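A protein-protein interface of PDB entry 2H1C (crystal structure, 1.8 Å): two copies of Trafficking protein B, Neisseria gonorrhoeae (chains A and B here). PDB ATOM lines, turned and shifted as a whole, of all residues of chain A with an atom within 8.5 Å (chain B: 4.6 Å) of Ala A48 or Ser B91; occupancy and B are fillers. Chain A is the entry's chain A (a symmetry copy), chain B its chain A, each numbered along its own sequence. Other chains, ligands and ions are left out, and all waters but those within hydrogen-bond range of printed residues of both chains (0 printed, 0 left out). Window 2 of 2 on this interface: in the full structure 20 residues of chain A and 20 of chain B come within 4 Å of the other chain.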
ATOM      1  N   ALA A  41      10.111  -3.454 -27.999  1.00  0.00           N
ATOM      2  CA  ALA A  41       9.978  -4.915 -27.929  1.00  0.00           C
ATOM      3  C   ALA A  41      10.980  -5.591 -28.871  1.00  0.00           C
ATOM      4  O   ALA A  41      11.587  -6.618 -28.524  1.00  0.00           O
ATOM      5  CB  ALA A  41       8.574  -5.331 -28.310  1.00  0.00           C
ATOM      6  N   GLU A  42      11.127  -5.042 -30.074  1.00  0.00           N
ATOM      7  CA  GLU A  42      12.051  -5.623 -31.047  1.00  0.00           C
ATOM      8  C   GLU A  42      13.499  -5.460 -30.600  1.00  0.00           C
ATOM      9  O   GLU A  42      14.313  -6.363 -30.810  1.00  0.00           O
ATOM     10  CB  GLU A  42      11.860  -4.997 -32.432  1.00  0.00           C
ATOM     11  CG  GLU A  42      10.418  -5.047 -32.932  1.00  0.00           C
ATOM     12  CD  GLU A  42      10.249  -4.444 -34.316  1.00  0.00           C
ATOM     13  OE1 GLU A  42      11.029  -3.517 -34.656  1.00  0.00           O
ATOM     14  OE2 GLU A  42       9.328  -4.881 -35.054  1.00  0.00           O
ATOM     15  N   LEU A  43      13.829  -4.313 -29.999  1.00  0.00           N
ATOM     16  CA  LEU A  43      15.189  -4.104 -29.495  1.00  0.00           C
ATOM     17  C   LEU A  43      15.465  -5.111 -28.384  1.00  0.00           C
ATOM     18  O   LEU A  43      16.508  -5.770 -28.375  1.00  0.00           O
ATOM     19  CB  LEU A  43      15.361  -2.683 -28.943  1.00  0.00           C
ATOM     20  CG  LEU A  43      15.318  -1.604 -30.020  1.00  0.00           C
ATOM     21  CD1 LEU A  43      15.267  -0.210 -29.395  1.00  0.00           C
ATOM     22  CD2 LEU A  43      16.545  -1.765 -30.901  1.00  0.00           C
ATOM     23  N   ARG A  44      14.532  -5.235 -27.445  1.00  0.00           N
ATOM     24  CA  ARG A  44      14.722  -6.178 -26.346  1.00  0.00           C
ATOM     25  C   ARG A  44      14.834  -7.621 -26.837  1.00  0.00           C
ATOM     26  O   ARG A  44      15.618  -8.393 -26.294  1.00  0.00           O
ATOM     27  CB  ARG A  44      13.586  -6.044 -25.316  1.00  0.00           C
ATOM     28  CG  ARG A  44      13.726  -4.811 -24.400  1.00  0.00           C
ATOM     29  CD  ARG A  44      12.441  -4.546 -23.605  1.00  0.00           C
ATOM     30  NE  ARG A  44      12.670  -3.622 -22.501  1.00  0.00           N
ATOM     31  CZ  ARG A  44      11.709  -2.968 -21.851  1.00  0.00           C
ATOM     32  NH1 ARG A  44      10.431  -3.127 -22.201  1.00  0.00           N
ATOM     33  NH2 ARG A  44      12.028  -2.164 -20.841  1.00  0.00           N
ATOM     34  N   LEU A  45      14.060  -7.984 -27.862  1.00  0.00           N
ATOM     35  CA  LEU A  45      14.099  -9.345 -28.396  1.00  0.00           C
ATOM     36  C   LEU A  45      15.451  -9.600 -29.063  1.00  0.00           C
ATOM     37  O   LEU A  45      16.069 -10.659 -28.878  1.00  0.00           O
ATOM     38  CB  LEU A  45      12.958  -9.540 -29.402  1.00  0.00           C
ATOM     39  CG  LEU A  45      12.925 -10.873 -30.150  1.00  0.00           C
ATOM     40  CD1 LEU A  45      12.937 -12.037 -29.161  1.00  0.00           C
ATOM     41  CD2 LEU A  45      11.686 -10.921 -31.036  1.00  0.00           C
ATOM     42  N   GLY A  46      15.912  -8.616 -29.833  1.00  0.00           N
ATOM     43  CA  GLY A  46      17.194  -8.734 -30.512  1.00  0.00           C
ATOM     44  C   GLY A  46      18.315  -8.984 -29.525  1.00  0.00           C
ATOM     45  O   GLY A  46      19.173  -9.855 -29.734  1.00  0.00           O
ATOM     46  N   VAL A  47      18.320  -8.227 -28.438  1.00  0.00           N
ATOM     47  CA  VAL A  47      19.356  -8.411 -27.428  1.00  0.00           C
ATOM     48  C   VAL A  47      19.244  -9.803 -26.807  1.00  0.00           C
ATOM     49  O   VAL A  47      20.251 -10.487 -26.623  1.00  0.00           O
ATOM     50  CB  VAL A  47      19.254  -7.366 -26.311  1.00  0.00           C
ATOM     51  CG1 VAL A  47      20.246  -7.694 -25.199  1.00  0.00           C
ATOM     52  CG2 VAL A  47      19.545  -5.972 -26.879  1.00  0.00           C
ATOM     53  N   ALA A  48      18.021 -10.231 -26.499  1.00  0.00           N
ATOM     54  CA  ALA A  48      17.830 -11.546 -25.889  1.00  0.00           C
ATOM     55  C   ALA A  48      18.197 -12.741 -26.777  1.00  0.00           C
ATOM     56  O   ALA A  48      18.360 -13.861 -26.276  1.00  0.00           O
ATOM     57  CB  ALA A  48      16.387 -11.690 -25.383  1.00  0.00           C
ATOM     58  N   LEU A  49      18.326 -12.513 -28.081  1.00  0.00           N
ATOM     59  CA  LEU A  49      18.668 -13.589 -29.012  1.00  0.00           C
ATOM     60  C   LEU A  49      20.148 -13.639 -29.372  1.00  0.00           C
ATOM     61  O   LEU A  49      20.560 -14.468 -30.189  1.00  0.00           O
ATOM     62  CB  LEU A  49      17.839 -13.460 -30.294  1.00  0.00           C
ATOM     63  CG  LEU A  49      16.345 -13.701 -30.070  1.00  0.00           C
ATOM     64  CD1 LEU A  49      15.545 -13.280 -31.293  1.00  0.00           C
ATOM     65  CD2 LEU A  49      16.136 -15.171 -29.737  1.00  0.00           C
ATOM     66  N   LEU A  50      20.954 -12.768 -28.767  1.00  0.00           N
ATOM     67  CA  LEU A  50      22.390 -12.768 -29.072  1.00  0.00           C
ATOM     68  C   LEU A  50      23.014 -14.113 -28.695  1.00  0.00           C
ATOM     69  O   LEU A  50      22.699 -14.674 -27.644  1.00  0.00           O
ATOM     70  CB  LEU A  50      23.105 -11.647 -28.319  1.00  0.00           C
ATOM     71  CG  LEU A  50      22.751 -10.218 -28.762  1.00  0.00           C
ATOM     72  CD1 LEU A  50      23.447  -9.225 -27.863  1.00  0.00           C
ATOM     73  CD2 LEU A  50      23.162  -9.997 -30.218  1.00  0.00           C
ATOM     74  N   LEU A  51      23.915 -14.607 -29.546  1.00  0.00           N
ATOM     75  CA  LEU A  51      24.580 -15.892 -29.308  1.00  0.00           C
ATOM     76  C   LEU A  51      25.713 -15.825 -28.274  1.00  0.00           C
ATOM     77  O   LEU A  51      26.086 -16.848 -27.687  1.00  0.00           O
ATOM     78  CB  LEU A  51      25.116 -16.457 -30.635  1.00  0.00           C
ATOM     79  CG  LEU A  51      24.094 -16.830 -31.728  1.00  0.00           C
ATOM     80  CD1 LEU A  51      24.830 -17.343 -32.973  1.00  0.00           C
ATOM     81  CD2 LEU A  51      23.138 -17.898 -31.217  1.00  0.00           C
ATOM     82  N   ASN A  52      26.250 -14.627 -28.053  1.00  0.00           N
ATOM     83  CA  ASN A  52      27.340 -14.403 -27.097  1.00  0.00           C
ATOM     84  C   ASN A  52      26.782 -13.993 -25.726  1.00  0.00           C
ATOM     85  O   ASN A  52      26.284 -12.882 -25.561  1.00  0.00           O
ATOM     86  CB  ASN A  52      28.270 -13.300 -27.640  1.00  0.00           C
ATOM     87  CG  ASN A  52      29.450 -13.012 -26.727  1.00  0.00           C
ATOM     88  OD1 ASN A  52      29.288 -12.811 -25.528  1.00  0.00           O
ATOM     89  ND2 ASN A  52      30.653 -12.979 -27.304  1.00  0.00           N
ATOM     90  N   LYS A  55      28.220 -10.646 -24.171  1.00  0.00           N
ATOM     91  CA  LYS A  55      27.707  -9.489 -24.890  1.00  0.00           C
ATOM     92  C   LYS A  55      26.247  -9.231 -24.547  1.00  0.00           C
ATOM     93  O   LYS A  55      25.847  -8.088 -24.327  1.00  0.00           O
ATOM     94  CB  LYS A  55      27.839  -9.703 -26.396  1.00  0.00           C
ATOM     95  CG  LYS A  55      27.406  -8.505 -27.232  1.00  0.00           C
ATOM     96  CD  LYS A  55      28.594  -7.840 -27.907  1.00  0.00           C
ATOM     97  CE  LYS A  55      29.297  -8.798 -28.861  1.00  0.00           C
ATOM     98  NZ  LYS A  55      30.388  -8.132 -29.627  1.00  0.00           N
ATOM     99  N   LYS A  56      25.448 -10.294 -24.517  1.00  0.00           N
ATOM    100  CA  LYS A  56      24.034 -10.161 -24.205  1.00  0.00           C
ATOM    101  C   LYS A  56      23.820  -9.534 -22.837  1.00  0.00           C
ATOM    102  O   LYS A  56      23.003  -8.630 -22.679  1.00  0.00           O
ATOM    103  CB  LYS A  56      23.346 -11.531 -24.244  1.00  0.00           C
ATOM    104  CG  LYS A  56      21.857 -11.460 -23.929  1.00  0.00           C
ATOM    105  CD  LYS A  56      21.183 -12.824 -23.996  1.00  0.00           C
ATOM    106  CE  LYS A  56      21.542 -13.680 -22.789  1.00  0.00           C
ATOM    107  NZ  LYS A  56      20.728 -14.933 -22.734  1.00  0.00           N
ATOM    108  N   ASN A  57      24.548 -10.021 -21.839  1.00  0.00           N
ATOM    109  CA  ASN A  57      24.401  -9.496 -20.487  1.00  0.00           C
ATOM    110  C   ASN A  57      24.752  -8.023 -20.411  1.00  0.00           C
ATOM    111  O   ASN A  57      24.013  -7.235 -19.827  1.00  0.00           O
ATOM    112  CB  ASN A  57      25.263 -10.292 -19.515  1.00  0.00           C
ATOM    113  CG  ASN A  57      24.598 -11.575 -19.084  1.00  0.00           C
ATOM    114  OD1 ASN A  57      24.166 -12.376 -19.917  1.00  0.00           O
ATOM    115  ND2 ASN A  57      24.504 -11.780 -17.775  1.00  0.00           N
ATOM    116  N   LEU A  59      24.891  -5.796 -22.958  1.00  0.00           N
ATOM    117  CA  LEU A  59      23.956  -4.986 -23.749  1.00  0.00           C
ATOM    118  C   LEU A  59      22.574  -4.897 -23.091  1.00  0.00           C
ATOM    119  O   LEU A  59      21.886  -3.874 -23.204  1.00  0.00           O
ATOM    120  CB  LEU A  59      23.854  -5.536 -25.184  1.00  0.00           C
ATOM    121  CG  LEU A  59      22.980  -4.800 -26.209  1.00  0.00           C
ATOM    122  CD1 LEU A  59      23.382  -3.327 -26.260  1.00  0.00           C
ATOM    123  CD2 LEU A  59      23.138  -5.430 -27.583  1.00  0.00           C
ATOM    124  N   HIS A  60      22.164  -5.958 -22.399  1.00  0.00           N
ATOM    125  CA  HIS A  60      20.879  -5.932 -21.718  1.00  0.00           C
ATOM    126  C   HIS A  60      20.943  -4.824 -20.660  1.00  0.00           C
ATOM    127  O   HIS A  60      20.043  -3.988 -20.564  1.00  0.00           O
ATOM    128  CB  HIS A  60      20.587  -7.292 -21.074  1.00  0.00           C
ATOM    129  CG  HIS A  60      19.397  -7.282 -20.169  1.00  0.00           C
ATOM    130  ND1 HIS A  60      19.463  -6.850 -18.860  1.00  0.00           N
ATOM    131  CD2 HIS A  60      18.099  -7.586 -20.397  1.00  0.00           C
ATOM    132  CE1 HIS A  60      18.256  -6.886 -18.326  1.00  0.00           C
ATOM    133  NE2 HIS A  60      17.408  -7.328 -19.237  1.00  0.00           N
ATOM    134  N   LEU A  63      20.951  -1.391 -22.383  1.00  0.00           N
ATOM    135  CA  LEU A  63      19.646  -1.044 -22.940  1.00  0.00           C
ATOM    136  C   LEU A  63      18.690  -0.585 -21.842  1.00  0.00           C
ATOM    137  O   LEU A  63      18.084   0.491 -21.921  1.00  0.00           O
ATOM    138  CB  LEU A  63      19.029  -2.245 -23.664  1.00  0.00           C
ATOM    139  CG  LEU A  63      17.647  -1.984 -24.281  1.00  0.00           C
ATOM    140  CD1 LEU A  63      17.742  -0.843 -25.311  1.00  0.00           C
ATOM    141  CD2 LEU A  63      17.145  -3.251 -24.944  1.00  0.00           C
ATOM    142  N   ALA B  87       9.585  -9.771 -25.325  1.00  0.00           N
ATOM    143  CA  ALA B  87      10.949 -10.183 -25.615  1.00  0.00           C
ATOM    144  C   ALA B  87      11.315 -11.428 -24.822  1.00  0.00           C
ATOM    145  O   ALA B  87      11.951 -12.338 -25.352  1.00  0.00           O
ATOM    146  CB  ALA B  87      11.916  -9.050 -25.303  1.00  0.00           C
ATOM    147  N   GLN B  88      10.899 -11.482 -23.559  1.00  0.00           N
ATOM    148  CA  GLN B  88      11.185 -12.642 -22.726  1.00  0.00           C
ATOM    149  C   GLN B  88      10.572 -13.909 -23.318  1.00  0.00           C
ATOM    150  O   GLN B  88      11.262 -14.911 -23.527  1.00  0.00           O
ATOM    151  CB  GLN B  88      10.651 -12.410 -21.311  1.00  0.00           C
ATOM    152  CG  GLN B  88      11.326 -11.224 -20.639  1.00  0.00           C
ATOM    153  CD  GLN B  88      10.911 -11.035 -19.197  1.00  0.00           C
ATOM    154  OE1 GLN B  88       9.735 -10.799 -18.895  1.00  0.00           O
ATOM    155  NE2 GLN B  88      11.882 -11.138 -18.290  1.00  0.00           N
ATOM    156  N   ILE B  89       9.275 -13.858 -23.597  1.00  0.00           N
ATOM    157  CA  ILE B  89       8.561 -15.001 -24.155  1.00  0.00           C
ATOM    158  C   ILE B  89       9.088 -15.465 -25.503  1.00  0.00           C
ATOM    159  O   ILE B  89       9.333 -16.656 -25.699  1.00  0.00           O
ATOM    160  CB  ILE B  89       7.047 -14.681 -24.315  1.00  0.00           C
ATOM    161  CG1 ILE B  89       6.375 -14.619 -22.945  1.00  0.00           C
ATOM    162  CG2 ILE B  89       6.389 -15.714 -25.214  1.00  0.00           C
ATOM    163  CD1 ILE B  89       4.888 -14.220 -23.015  1.00  0.00           C
ATOM    164  N   ARG B  90       9.253 -14.546 -26.446  1.00  0.00           N
ATOM    165  CA  ARG B  90       9.741 -14.940 -27.771  1.00  0.00           C
ATOM    166  C   ARG B  90      11.181 -15.453 -27.764  1.00  0.00           C
ATOM    167  O   ARG B  90      11.507 -16.408 -28.483  1.00  0.00           O
ATOM    168  CB  ARG B  90       9.623 -13.788 -28.764  1.00  0.00           C
ATOM    169  CG  ARG B  90       8.192 -13.461 -29.111  1.00  0.00           C
ATOM    170  CD  ARG B  90       8.108 -12.897 -30.506  1.00  0.00           C
ATOM    171  NE  ARG B  90       8.586 -13.838 -31.510  1.00  0.00           N
ATOM    172  CZ  ARG B  90       8.913 -13.496 -32.755  1.00  0.00           C
ATOM    173  NH1 ARG B  90       8.815 -12.233 -33.153  1.00  0.00           N
ATOM    174  NH2 ARG B  90       9.350 -14.420 -33.604  1.00  0.00           N
ATOM    175  N   SER B  91      12.047 -14.842 -26.962  1.00  0.00           N
ATOM    176  CA  SER B  91      13.428 -15.296 -26.918  1.00  0.00           C
ATOM    177  C   SER B  91      13.504 -16.684 -26.280  1.00  0.00           C
ATOM    178  O   SER B  91      14.207 -17.575 -26.782  1.00  0.00           O
ATOM    179  CB  SER B  91      14.306 -14.302 -26.148  1.00  0.00           C
ATOM    180  OG  SER B  91      13.989 -14.288 -24.770  1.00  0.00           O
ATOM    181  N   TYR B  92      12.766 -16.881 -25.189  1.00  0.00           N
ATOM    182  CA  TYR B  92      12.765 -18.165 -24.504  1.00  0.00           C
ATOM    183  C   TYR B  92      12.298 -19.267 -25.451  1.00  0.00           C
ATOM    184  O   TYR B  92      12.898 -20.340 -25.515  1.00  0.00           O
ATOM    185  CB  TYR B  92      11.843 -18.135 -23.288  1.00  0.00           C
ATOM    186  CG  TYR B  92      12.001 -19.356 -22.406  1.00  0.00           C
ATOM    187  CD1 TYR B  92      12.977 -19.398 -21.412  1.00  0.00           C
ATOM    188  CD2 TYR B  92      11.194 -20.477 -22.583  1.00  0.00           C
ATOM    189  CE1 TYR B  92      13.145 -20.525 -20.610  1.00  0.00           C
ATOM    190  CE2 TYR B  92      11.356 -21.614 -21.791  1.00  0.00           C
ATOM    191  CZ  TYR B  92      12.331 -21.626 -20.806  1.00  0.00           C
ATOM    192  OH  TYR B  92      12.488 -22.736 -20.010  1.00  0.00           O
ATOM    193  N   ALA B  93      11.224 -19.005 -26.185  1.00  0.00           N
ATOM    194  CA  ALA B  93      10.713 -19.999 -27.125  1.00  0.00           C
ATOM    195  C   ALA B  93      11.777 -20.319 -28.167  1.00  0.00           C
ATOM    196  O   ALA B  93      12.018 -21.488 -28.484  1.00  0.00           O
ATOM    197  CB  ALA B  93       9.444 -19.486 -27.805  1.00  0.00           C
ATOM    198  N   LYS B  94      12.415 -19.279 -28.700  1.00  0.00           N
ATOM    199  CA  LYS B  94      13.450 -19.459 -29.710  1.00  0.00           C
ATOM    200  C   LYS B  94      14.650 -20.257 -29.196  1.00  0.00           C
ATOM    201  O   LYS B  94      15.146 -21.153 -29.884  1.00  0.00           O
ATOM    202  CB  LYS B  94      13.931 -18.097 -30.220  1.00  0.00           C
ATOM    203  CG  LYS B  94      14.014 -17.993 -31.733  1.00  0.00           C
ATOM    204  CD  LYS B  94      12.641 -18.108 -32.370  1.00  0.00           C
ATOM    205  CE  LYS B  94      12.715 -17.912 -33.877  1.00  0.00           C
ATOM    206  NZ  LYS B  94      13.281 -16.577 -34.211  1.00  0.00           N
ATOM    207  N   THR B  95      15.117 -19.944 -27.988  1.00  0.00           N
ATOM    208  CA  THR B  95      16.272 -20.652 -27.445  1.00  0.00           C
ATOM    209  C   THR B  95      15.912 -22.061 -26.977  1.00  0.00           C
ATOM    210  O   THR B  95      16.782 -22.797 -26.502  1.00  0.00           O
ATOM    211  CB  THR B  95      16.916 -19.889 -26.275  1.00  0.00           C
ATOM    212  OG1 THR B  95      15.968 -19.749 -25.208  1.00  0.00           O
ATOM    213  CG2 THR B  95      17.385 -18.510 -26.738  1.00  0.00           C
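The backbone carbonyl oxygen (O) of Ala B87 sits at hydrogen-bond distance from the side-chain hydroxyl (OG) of Ser B91, 2.9 Å away.
O of Gln B88 is in hydrogen-bond range of OG of Ser B91.
OG1 of Thr B95 is in hydrogen-bond range of O of Ser B91 (3.2 Å).
Arg A44 touches Ala B87 (CB to CB, 3.4 Å).
Leu A45 touches Ala B87 (N to CB, 3.5 Å).
Leu A45 touches Arg B90 (CD1 to CB, 3.8 Å).
Leu A45 touches Ser B91.
CB of Ser B91 touches CB of Ala A48, 3.4 Å away.
CA of Ser B91 touches CD2 of Leu A49, at 3.9 Å.
Leu A49 touches Lys B94.
Of chain B, only Ser B91 comes within 4 Å of Ala A48.
Of the printed residues of chain A, Ser B91 touches Leu A45 (3.7 Å), Ala A48 (3.4 Å) and Leu A49 (3.9 Å).
Printed residues of chain B within 4 Å of Leu A49: Ser B91 and Lys B94.
Printed residues of chain A within 4 Å of Lys B94: Leu A49 (3.7 Å).
Printed residues of chain A within 4 Å of Arg B90: Leu A45 (3.8 Å).
Printed residues of chain B within 4 Å of Arg A44: Ala B87 (3.4 Å).
Glu A42 touches none of the printed residues of chain B.
The nearest residue of chain B that does not touch Ala A48 is Ala B87 (4.5 Å).
The nearest residue of chain A that does not touch Ser B91 is Arg A44 (6.1 Å).
Of the 18 printed residues of chain A, 4 touch a printed residue of chain B.
Hydrophobic or aromatic side chains of chain A within 4 Å of the printed part of chain B: Leu A45, Ala A48 and Leu A49.
Among the printed residues, 7 pairs touch across the chains.
Among the printed residues, no Asp or Glu carboxylate lies within 4 Å of a Lys or Arg side-chain nitrogen of the other chain.
No position is printed for both chains.
Of the 7 pairs that touch across the chains among the printed residues, none has its exchanged pair printed and touching as well.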
